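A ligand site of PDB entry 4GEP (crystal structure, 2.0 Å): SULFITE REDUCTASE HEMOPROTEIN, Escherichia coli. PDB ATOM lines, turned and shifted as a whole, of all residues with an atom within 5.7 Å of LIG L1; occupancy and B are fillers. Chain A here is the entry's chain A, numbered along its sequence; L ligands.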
ATOM      1  N   CYS A 361     -20.245   6.263  -7.852  1.00  0.00           N
ATOM      2  CA  CYS A 361     -20.148   6.778  -6.488  1.00  0.00           C
ATOM      3  C   CYS A 361     -19.398   5.759  -5.639  1.00  0.00           C
ATOM      4  O   CYS A 361     -19.099   4.660  -6.106  1.00  0.00           O
ATOM      5  CB  CYS A 361     -21.548   6.991  -5.886  1.00  0.00           C
ATOM      6  SG  CYS A 361     -22.505   5.455  -5.656  1.00  0.00           S
ATOM      7  N   VAL A 362     -19.110   6.112  -4.384  1.00  0.00           N
ATOM      8  CA  VAL A 362     -18.407   5.214  -3.493  1.00  0.00           C
ATOM      9  C   VAL A 362     -19.195   3.907  -3.234  1.00  0.00           C
ATOM     10  O   VAL A 362     -18.719   2.798  -3.529  1.00  0.00           O
ATOM     11  CB  VAL A 362     -18.102   5.897  -2.185  1.00  0.00           C
ATOM     12  CG1 VAL A 362     -17.478   4.917  -1.240  1.00  0.00           C
ATOM     13  CG2 VAL A 362     -17.158   7.052  -2.425  1.00  0.00           C
ATOM     14  N   SER A 363     -20.412   4.044  -2.703  1.00  0.00           N
ATOM     15  CA  SER A 363     -21.258   2.888  -2.419  1.00  0.00           C
ATOM     16  C   SER A 363     -20.540   1.954  -1.432  1.00  0.00           C
ATOM     17  O   SER A 363     -19.823   2.438  -0.550  1.00  0.00           O
ATOM     18  CB  SER A 363     -21.600   2.169  -3.724  1.00  0.00           C
ATOM     19  OG  SER A 363     -22.461   1.068  -3.477  1.00  0.00           O
ATOM     20  N   PHE A 364     -20.789   0.643  -1.510  1.00  0.00           N
ATOM     21  CA  PHE A 364     -20.117  -0.298  -0.630  1.00  0.00           C
ATOM     22  C   PHE A 364     -18.632  -0.182  -0.873  1.00  0.00           C
ATOM     23  O   PHE A 364     -18.197   0.025  -1.997  1.00  0.00           O
ATOM     24  CB  PHE A 364     -20.553  -1.735  -0.910  1.00  0.00           C
ATOM     25  CG  PHE A 364     -22.002  -1.982  -0.682  1.00  0.00           C
ATOM     26  CD1 PHE A 364     -22.548  -1.845   0.588  1.00  0.00           C
ATOM     27  CD2 PHE A 364     -22.845  -2.290  -1.738  1.00  0.00           C
ATOM     28  CE1 PHE A 364     -23.901  -2.028   0.796  1.00  0.00           C
ATOM     29  CE2 PHE A 364     -24.204  -2.462  -1.544  1.00  0.00           C
ATOM     30  CZ  PHE A 364     -24.727  -2.334  -0.274  1.00  0.00           C
ATOM     31  N   CYS A 367     -20.329   3.136   2.311  1.00  0.00           N
ATOM     32  CA  CYS A 367     -21.563   3.874   2.413  1.00  0.00           C
ATOM     33  C   CYS A 367     -22.658   3.089   3.087  1.00  0.00           C
ATOM     34  O   CYS A 367     -22.955   1.974   2.690  1.00  0.00           O
ATOM     35  CB  CYS A 367     -22.036   4.314   1.051  1.00  0.00           C
ATOM     36  SG  CYS A 367     -23.452   5.452   1.134  1.00  0.00           S
ATOM     37  N   PRO A 368     -23.318   3.686   4.090  1.00  0.00           N
ATOM     38  CA  PRO A 368     -24.403   3.022   4.813  1.00  0.00           C
ATOM     39  C   PRO A 368     -25.750   3.044   4.083  1.00  0.00           C
ATOM     40  O   PRO A 368     -26.669   2.269   4.403  1.00  0.00           O
ATOM     41  CB  PRO A 368     -24.469   3.822   6.109  1.00  0.00           C
ATOM     42  CG  PRO A 368     -24.093   5.204   5.648  1.00  0.00           C
ATOM     43  CD  PRO A 368     -22.919   4.935   4.752  1.00  0.00           C
ATOM     44  N   LEU A 369     -25.858   3.901   3.079  1.00  0.00           N
ATOM     45  CA  LEU A 369     -27.109   4.022   2.354  1.00  0.00           C
ATOM     46  C   LEU A 369     -27.100   3.243   1.067  1.00  0.00           C
ATOM     47  O   LEU A 369     -28.121   3.175   0.373  1.00  0.00           O
ATOM     48  CB  LEU A 369     -27.372   5.506   2.055  1.00  0.00           C
ATOM     49  CG  LEU A 369     -27.161   6.443   3.228  1.00  0.00           C
ATOM     50  CD1 LEU A 369     -27.460   7.869   2.794  1.00  0.00           C
ATOM     51  CD2 LEU A 369     -28.072   6.036   4.403  1.00  0.00           C
ATOM     52  N   ALA A 370     -25.971   2.626   0.771  1.00  0.00           N
ATOM     53  CA  ALA A 370     -25.817   1.877  -0.468  1.00  0.00           C
ATOM     54  C   ALA A 370     -26.805   0.729  -0.662  1.00  0.00           C
ATOM     55  O   ALA A 370     -27.074  -0.021   0.273  1.00  0.00           O
ATOM     56  CB  ALA A 370     -24.384   1.380  -0.583  1.00  0.00           C
ATOM     57  N   MET A 371     -27.289   0.557  -1.890  1.00  0.00           N
ATOM     58  CA  MET A 371     -28.210  -0.521  -2.204  1.00  0.00           C
ATOM     59  C   MET A 371     -27.558  -1.527  -3.155  1.00  0.00           C
ATOM     60  O   MET A 371     -27.809  -2.724  -3.077  1.00  0.00           O
ATOM     61  CB  MET A 371     -29.486   0.040  -2.820  1.00  0.00           C
ATOM     62  CG  MET A 371     -30.211   1.077  -1.944  1.00  0.00           C
ATOM     63  SD  MET A 371     -31.698   1.677  -2.757  1.00  0.00           S
ATOM     64  CE  MET A 371     -32.640   2.372  -1.389  1.00  0.00           C
ATOM     65  N   ALA A 372     -26.715  -1.028  -4.049  1.00  0.00           N
ATOM     66  CA  ALA A 372     -26.035  -1.880  -5.018  1.00  0.00           C
ATOM     67  C   ALA A 372     -24.616  -1.336  -5.168  1.00  0.00           C
ATOM     68  O   ALA A 372     -24.375  -0.178  -4.838  1.00  0.00           O
ATOM     69  CB  ALA A 372     -26.754  -1.835  -6.337  1.00  0.00           C
ATOM     70  N   ALA A 374     -21.209   0.162  -6.753  1.00  0.00           N
ATOM     71  CA  ALA A 374     -21.010   1.198  -7.748  1.00  0.00           C
ATOM     72  C   ALA A 374     -19.527   1.275  -8.080  1.00  0.00           C
ATOM     73  O   ALA A 374     -19.082   0.781  -9.116  1.00  0.00           O
ATOM     74  CB  ALA A 374     -21.532   2.530  -7.241  1.00  0.00           C
ATOM     75  N   THR A 404     -24.808   4.827  -9.924  1.00  0.00           N
ATOM     76  CA  THR A 404     -24.958   5.377  -8.608  1.00  0.00           C
ATOM     77  C   THR A 404     -25.559   4.226  -7.773  1.00  0.00           C
ATOM     78  O   THR A 404     -26.386   3.456  -8.256  1.00  0.00           O
ATOM     79  CB  THR A 404     -25.812   6.688  -8.698  1.00  0.00           C
ATOM     80  OG1 THR A 404     -25.600   7.482  -7.535  1.00  0.00           O
ATOM     81  CG2 THR A 404     -27.277   6.413  -8.859  1.00  0.00           C
ATOM     82  N   GLY A 405     -25.024   4.015  -6.589  1.00  0.00           N
ATOM     83  CA  GLY A 405     -25.456   2.904  -5.755  1.00  0.00           C
ATOM     84  C   GLY A 405     -26.805   2.935  -5.053  1.00  0.00           C
ATOM     85  O   GLY A 405     -27.172   1.971  -4.408  1.00  0.00           O
ATOM     86  N   CYS A 406     -27.510   4.046  -5.165  1.00  0.00           N
ATOM     87  CA  CYS A 406     -28.813   4.200  -4.548  1.00  0.00           C
ATOM     88  C   CYS A 406     -29.347   5.493  -5.171  1.00  0.00           C
ATOM     89  O   CYS A 406     -28.583   6.244  -5.773  1.00  0.00           O
ATOM     90  CB  CYS A 406     -28.705   4.246  -3.004  1.00  0.00           C
ATOM     91  SG  CYS A 406     -28.341   5.845  -2.229  1.00  0.00           S
ATOM     92  N   PRO A 407     -30.661   5.767  -5.045  1.00  0.00           N
ATOM     93  CA  PRO A 407     -31.274   6.967  -5.623  1.00  0.00           C
ATOM     94  C   PRO A 407     -30.800   8.335  -5.159  1.00  0.00           C
ATOM     95  O   PRO A 407     -31.154   9.326  -5.787  1.00  0.00           O
ATOM     96  CB  PRO A 407     -32.757   6.721  -5.396  1.00  0.00           C
ATOM     97  CG  PRO A 407     -32.760   6.030  -4.067  1.00  0.00           C
ATOM     98  CD  PRO A 407     -31.652   5.012  -4.239  1.00  0.00           C
ATOM     99  N   ASN A 408     -30.001   8.397  -4.104  1.00  0.00           N
ATOM    100  CA  ASN A 408     -29.461   9.676  -3.629  1.00  0.00           C
ATOM    101  C   ASN A 408     -28.732  10.322  -4.799  1.00  0.00           C
ATOM    102  O   ASN A 408     -28.665  11.546  -4.905  1.00  0.00           O
ATOM    103  CB  ASN A 408     -28.545   9.485  -2.418  1.00  0.00           C
ATOM    104  CG  ASN A 408     -29.321   9.298  -1.116  1.00  0.00           C
ATOM    105  OD1 ASN A 408     -30.450   9.755  -0.995  1.00  0.00           O
ATOM    106  ND2 ASN A 408     -28.726   8.645  -0.147  1.00  0.00           N
ATOM    107  N   GLY A 409     -28.139   9.485  -5.653  1.00  0.00           N
ATOM    108  CA  GLY A 409     -27.530   9.998  -6.876  1.00  0.00           C
ATOM    109  C   GLY A 409     -26.151  10.601  -6.927  1.00  0.00           C
ATOM    110  O   GLY A 409     -25.832  11.293  -7.903  1.00  0.00           O
ATOM    111  N   CYS A 410     -25.313  10.277  -5.959  1.00  0.00           N
ATOM    112  CA  CYS A 410     -23.949  10.784  -5.880  1.00  0.00           C
ATOM    113  C   CYS A 410     -23.112  10.552  -7.166  1.00  0.00           C
ATOM    114  O   CYS A 410     -22.311  11.400  -7.557  1.00  0.00           O
ATOM    115  CB  CYS A 410     -23.267  10.184  -4.654  1.00  0.00           C
ATOM    116  SG  CYS A 410     -24.182  10.529  -3.114  1.00  0.00           S
ATOM    117  N   GLY A 411     -23.378   9.467  -7.865  1.00  0.00           N
ATOM    118  CA  GLY A 411     -22.648   9.155  -9.076  1.00  0.00           C
ATOM    119  C   GLY A 411     -23.110   9.947 -10.284  1.00  0.00           C
ATOM    120  O   GLY A 411     -22.544   9.779 -11.373  1.00  0.00           O
HETATM  121 FE1  LIG L   1     -23.656   6.052  -3.782  1.00  0.00          FE
HETATM  122 FE2  LIG L   1     -23.899   5.998  -1.035  1.00  0.00          FE
HETATM  123 FE3  LIG L   1     -26.101   6.243  -2.466  1.00  0.00          FE
HETATM  124 FE4  LIG L   1     -24.259   8.279  -2.602  1.00  0.00          FE
HETATM  125  S1  LIG L   1     -25.449   7.614  -0.748  1.00  0.00           S
HETATM  126  S2  LIG L   1     -25.456   7.343  -4.325  1.00  0.00           S
HETATM  127  S3  LIG L   1     -22.322   7.069  -2.396  1.00  0.00           S
HETATM  128  S4  LIG L   1     -24.644   4.491  -2.415  1.00  0.00           S
HETATM  129 FE1  LG2 L   2     -23.353  12.249  -1.964  1.00  0.00          FE
HETATM  130  C1  LG2 L   2     -24.821  11.235   0.843  1.00  0.00           C
HETATM  131  C2  LG2 L   2     -20.625  10.297  -1.212  1.00  0.00           C
HETATM  132  C3  LG2 L   2     -21.658  13.706  -4.476  1.00  0.00           C
HETATM  133  C4  LG2 L   2     -26.305  13.340  -3.233  1.00  0.00           C
HETATM  134  N1  LG2 L   2     -22.824  10.973  -0.428  1.00  0.00           N
HETATM  135  C5  LG2 L   2     -23.560  10.758   0.707  1.00  0.00           C
HETATM  136  C6  LG2 L   2     -22.731  10.039   1.720  1.00  0.00           C
HETATM  137  C7  LG2 L   2     -21.996  11.173   2.487  1.00  0.00           C
HETATM  138  C8  LG2 L   2     -23.545   9.068   2.595  1.00  0.00           C
HETATM  139  C9  LG2 L   2     -24.037   9.580   3.953  1.00  0.00           C
HETATM  140  O1  LG2 L   2     -24.949  10.430   3.987  1.00  0.00           O
HETATM  141  O2  LG2 L   2     -23.515   9.149   4.983  1.00  0.00           O
HETATM  142  C10 LG2 L   2     -21.852   9.275   0.814  1.00  0.00           C
HETATM  143  C11 LG2 L   2     -20.569   8.902   1.402  1.00  0.00           C
HETATM  144  C12 LG2 L   2     -20.228   7.522   0.896  1.00  0.00           C
HETATM  145  C13 LG2 L   2     -18.861   7.039   1.344  1.00  0.00           C
HETATM  146  O3  LG2 L   2     -18.771   5.949   1.951  1.00  0.00           O
HETATM  147  O4  LG2 L   2     -17.853   7.723   1.071  1.00  0.00           O
HETATM  148  C14 LG2 L   2     -21.695  10.239  -0.332  1.00  0.00           C
HETATM  149  N2  LG2 L   2     -21.462  12.038  -2.696  1.00  0.00           N
HETATM  150  C15 LG2 L   2     -20.509  11.121  -2.310  1.00  0.00           C
HETATM  151  C16 LG2 L   2     -19.321  11.226  -3.247  1.00  0.00           C
HETATM  152  C17 LG2 L   2     -18.031  10.920  -2.466  1.00  0.00           C
HETATM  153  C18 LG2 L   2     -19.554  10.314  -4.453  1.00  0.00           C
HETATM  154  C19 LG2 L   2     -18.353  10.021  -5.294  1.00  0.00           C
HETATM  155  O5  LG2 L   2     -18.052   8.852  -5.549  1.00  0.00           O
HETATM  156  O6  LG2 L   2     -17.670  10.964  -5.711  1.00  0.00           O
HETATM  157  C20 LG2 L   2     -19.462  12.725  -3.607  1.00  0.00           C
HETATM  158  C21 LG2 L   2     -18.957  13.609  -2.495  1.00  0.00           C
HETATM  159  C22 LG2 L   2     -19.123  15.039  -2.927  1.00  0.00           C
HETATM  160  C23 LG2 L   2     -18.343  16.000  -2.060  1.00  0.00           C
HETATM  161  O7  LG2 L   2     -17.110  15.896  -2.031  1.00  0.00           O
HETATM  162  O8  LG2 L   2     -18.962  16.883  -1.443  1.00  0.00           O
HETATM  163  C24 LG2 L   2     -20.947  12.850  -3.700  1.00  0.00           C
HETATM  164  N3  LG2 L   2     -23.894  13.357  -3.570  1.00  0.00           N
HETATM  165  C25 LG2 L   2     -23.025  13.920  -4.457  1.00  0.00           C
HETATM  166  C26 LG2 L   2     -23.837  14.277  -5.683  1.00  0.00           C
HETATM  167  C27 LG2 L   2     -23.263  14.777  -6.993  1.00  0.00           C
HETATM  168  C28 LG2 L   2     -22.659  16.169  -6.945  1.00  0.00           C
HETATM  169  O9  LG2 L   2     -22.881  16.901  -5.965  1.00  0.00           O
HETATM  170  O10 LG2 L   2     -21.935  16.544  -7.870  1.00  0.00           O
HETATM  171  C29 LG2 L   2     -25.163  14.092  -5.391  1.00  0.00           C
HETATM  172  C30 LG2 L   2     -26.311  14.315  -6.316  1.00  0.00           C
HETATM  173  C31 LG2 L   2     -26.720  15.755  -6.550  1.00  0.00           C
HETATM  174  C32 LG2 L   2     -27.625  16.302  -5.470  1.00  0.00           C
HETATM  175  O11 LG2 L   2     -27.116  16.665  -4.404  1.00  0.00           O
HETATM  176  O12 LG2 L   2     -28.840  16.402  -5.684  1.00  0.00           O
HETATM  177  C33 LG2 L   2     -25.177  13.603  -3.989  1.00  0.00           C
HETATM  178  N4  LG2 L   2     -25.268  12.284  -1.303  1.00  0.00           N
HETATM  179  C34 LG2 L   2     -26.363  12.731  -1.988  1.00  0.00           C
HETATM  180  C35 LG2 L   2     -27.557  12.623  -1.058  1.00  0.00           C
HETATM  181  C36 LG2 L   2     -28.929  13.128  -1.419  1.00  0.00           C
HETATM  182  C37 LG2 L   2     -29.123  14.558  -0.926  1.00  0.00           C
HETATM  183  C38 LG2 L   2     -30.484  15.089  -1.226  1.00  0.00           C
HETATM  184  O13 LG2 L   2     -30.606  16.302  -1.498  1.00  0.00           O
HETATM  185  O14 LG2 L   2     -31.436  14.300  -1.193  1.00  0.00           O
HETATM  186  C39 LG2 L   2     -27.087  12.057   0.119  1.00  0.00           C
HETATM  187  C40 LG2 L   2     -27.798  11.606   1.369  1.00  0.00           C
HETATM  188  C41 LG2 L   2     -28.310  12.751   2.210  1.00  0.00           C
HETATM  189  O15 LG2 L   2     -27.599  13.759   2.342  1.00  0.00           O
HETATM  190  O16 LG2 L   2     -29.427  12.629   2.740  1.00  0.00           O
HETATM  191  C42 LG2 L   2     -25.618  11.899  -0.027  1.00  0.00           C
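The backbone NH of Cys 410 sits close to a sulfur (S2) of LIG L1, at 3.4 Å. OG1 of Thr 404 sits close to S2 of LIG L1 (3.2 Å). FE4 of LIG L1 is bound by SG of Cys 410 (2.3 Å). The backbone NH (N) of Ser 363 lies close to a sulfur (S3) of LIG L1 (3.6 Å). The side-chain sulfur (SG) of Cys 410 is bound to an iron atom (FE1) of LG2 L2 (2.2 Å). An iron atom (FE2) of LIG L1 is bound by the side-chain sulfur of Cys 367 (2.3 Å). N of Gly 409 lies close to S2 of LIG L1 (3.7 Å). The side-chain amide nitrogen of Asn 408 lies close to a sulfur (S1) of LIG L1 (3.5 Å). SG of Cys 406 is bound to FE3 of LIG L1, at 2.3 Å. An oxygen (O5) of LG2 L2 is in hydrogen-bond range of the backbone NH of Val 362 (3.2 Å). The side-chain sulfur (SG) of Cys 361 is bound to an iron atom (FE1) of LIG L1, at 2.3 Å. The backbone NH (N) of Cys 367 sits at hydrogen-bond distance from an oxygen (O3) of LG2 L2 (3.2 Å).
Merely in contact with LIG L1: Ala 370, Gly 405, Val 362 and Leu 369. Hydrophobic or aromatic side chains that line LIG L1: Leu 369 and Ala 370. Of the 19 residues printed, 12 come within 4 Å of LIG L1.
N of Cys 410 sits at hydrogen-bond distance from OG1 of Thr 404 (3.2 Å). The side-chain hydroxyl (OG) of Ser 363 lies within hydrogen-bond range of the backbone carbonyl oxygen (O) of Ala 372 (2.7 Å). The side-chain sulfur (SG) of Cys 367 sits close to the backbone NH (N) of Leu 369, at 3.5 Å. The backbone NH of Gly 411 sits at hydrogen-bond distance from the side-chain hydroxyl of Thr 404. The backbone NH (N) of Met 371 sits at hydrogen-bond distance from the backbone carbonyl oxygen (O) of Gly 405. The side-chain sulfur (SG) of Cys 406 sits close to the side-chain amide nitrogen (ND2) of Asn 408, 3.5 Å away. The side-chain sulfur of Cys 361 lies close to the backbone NH of Gly 405. N of Ala 372 lies within hydrogen-bond range of O of Gly 405 (3.1 Å).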
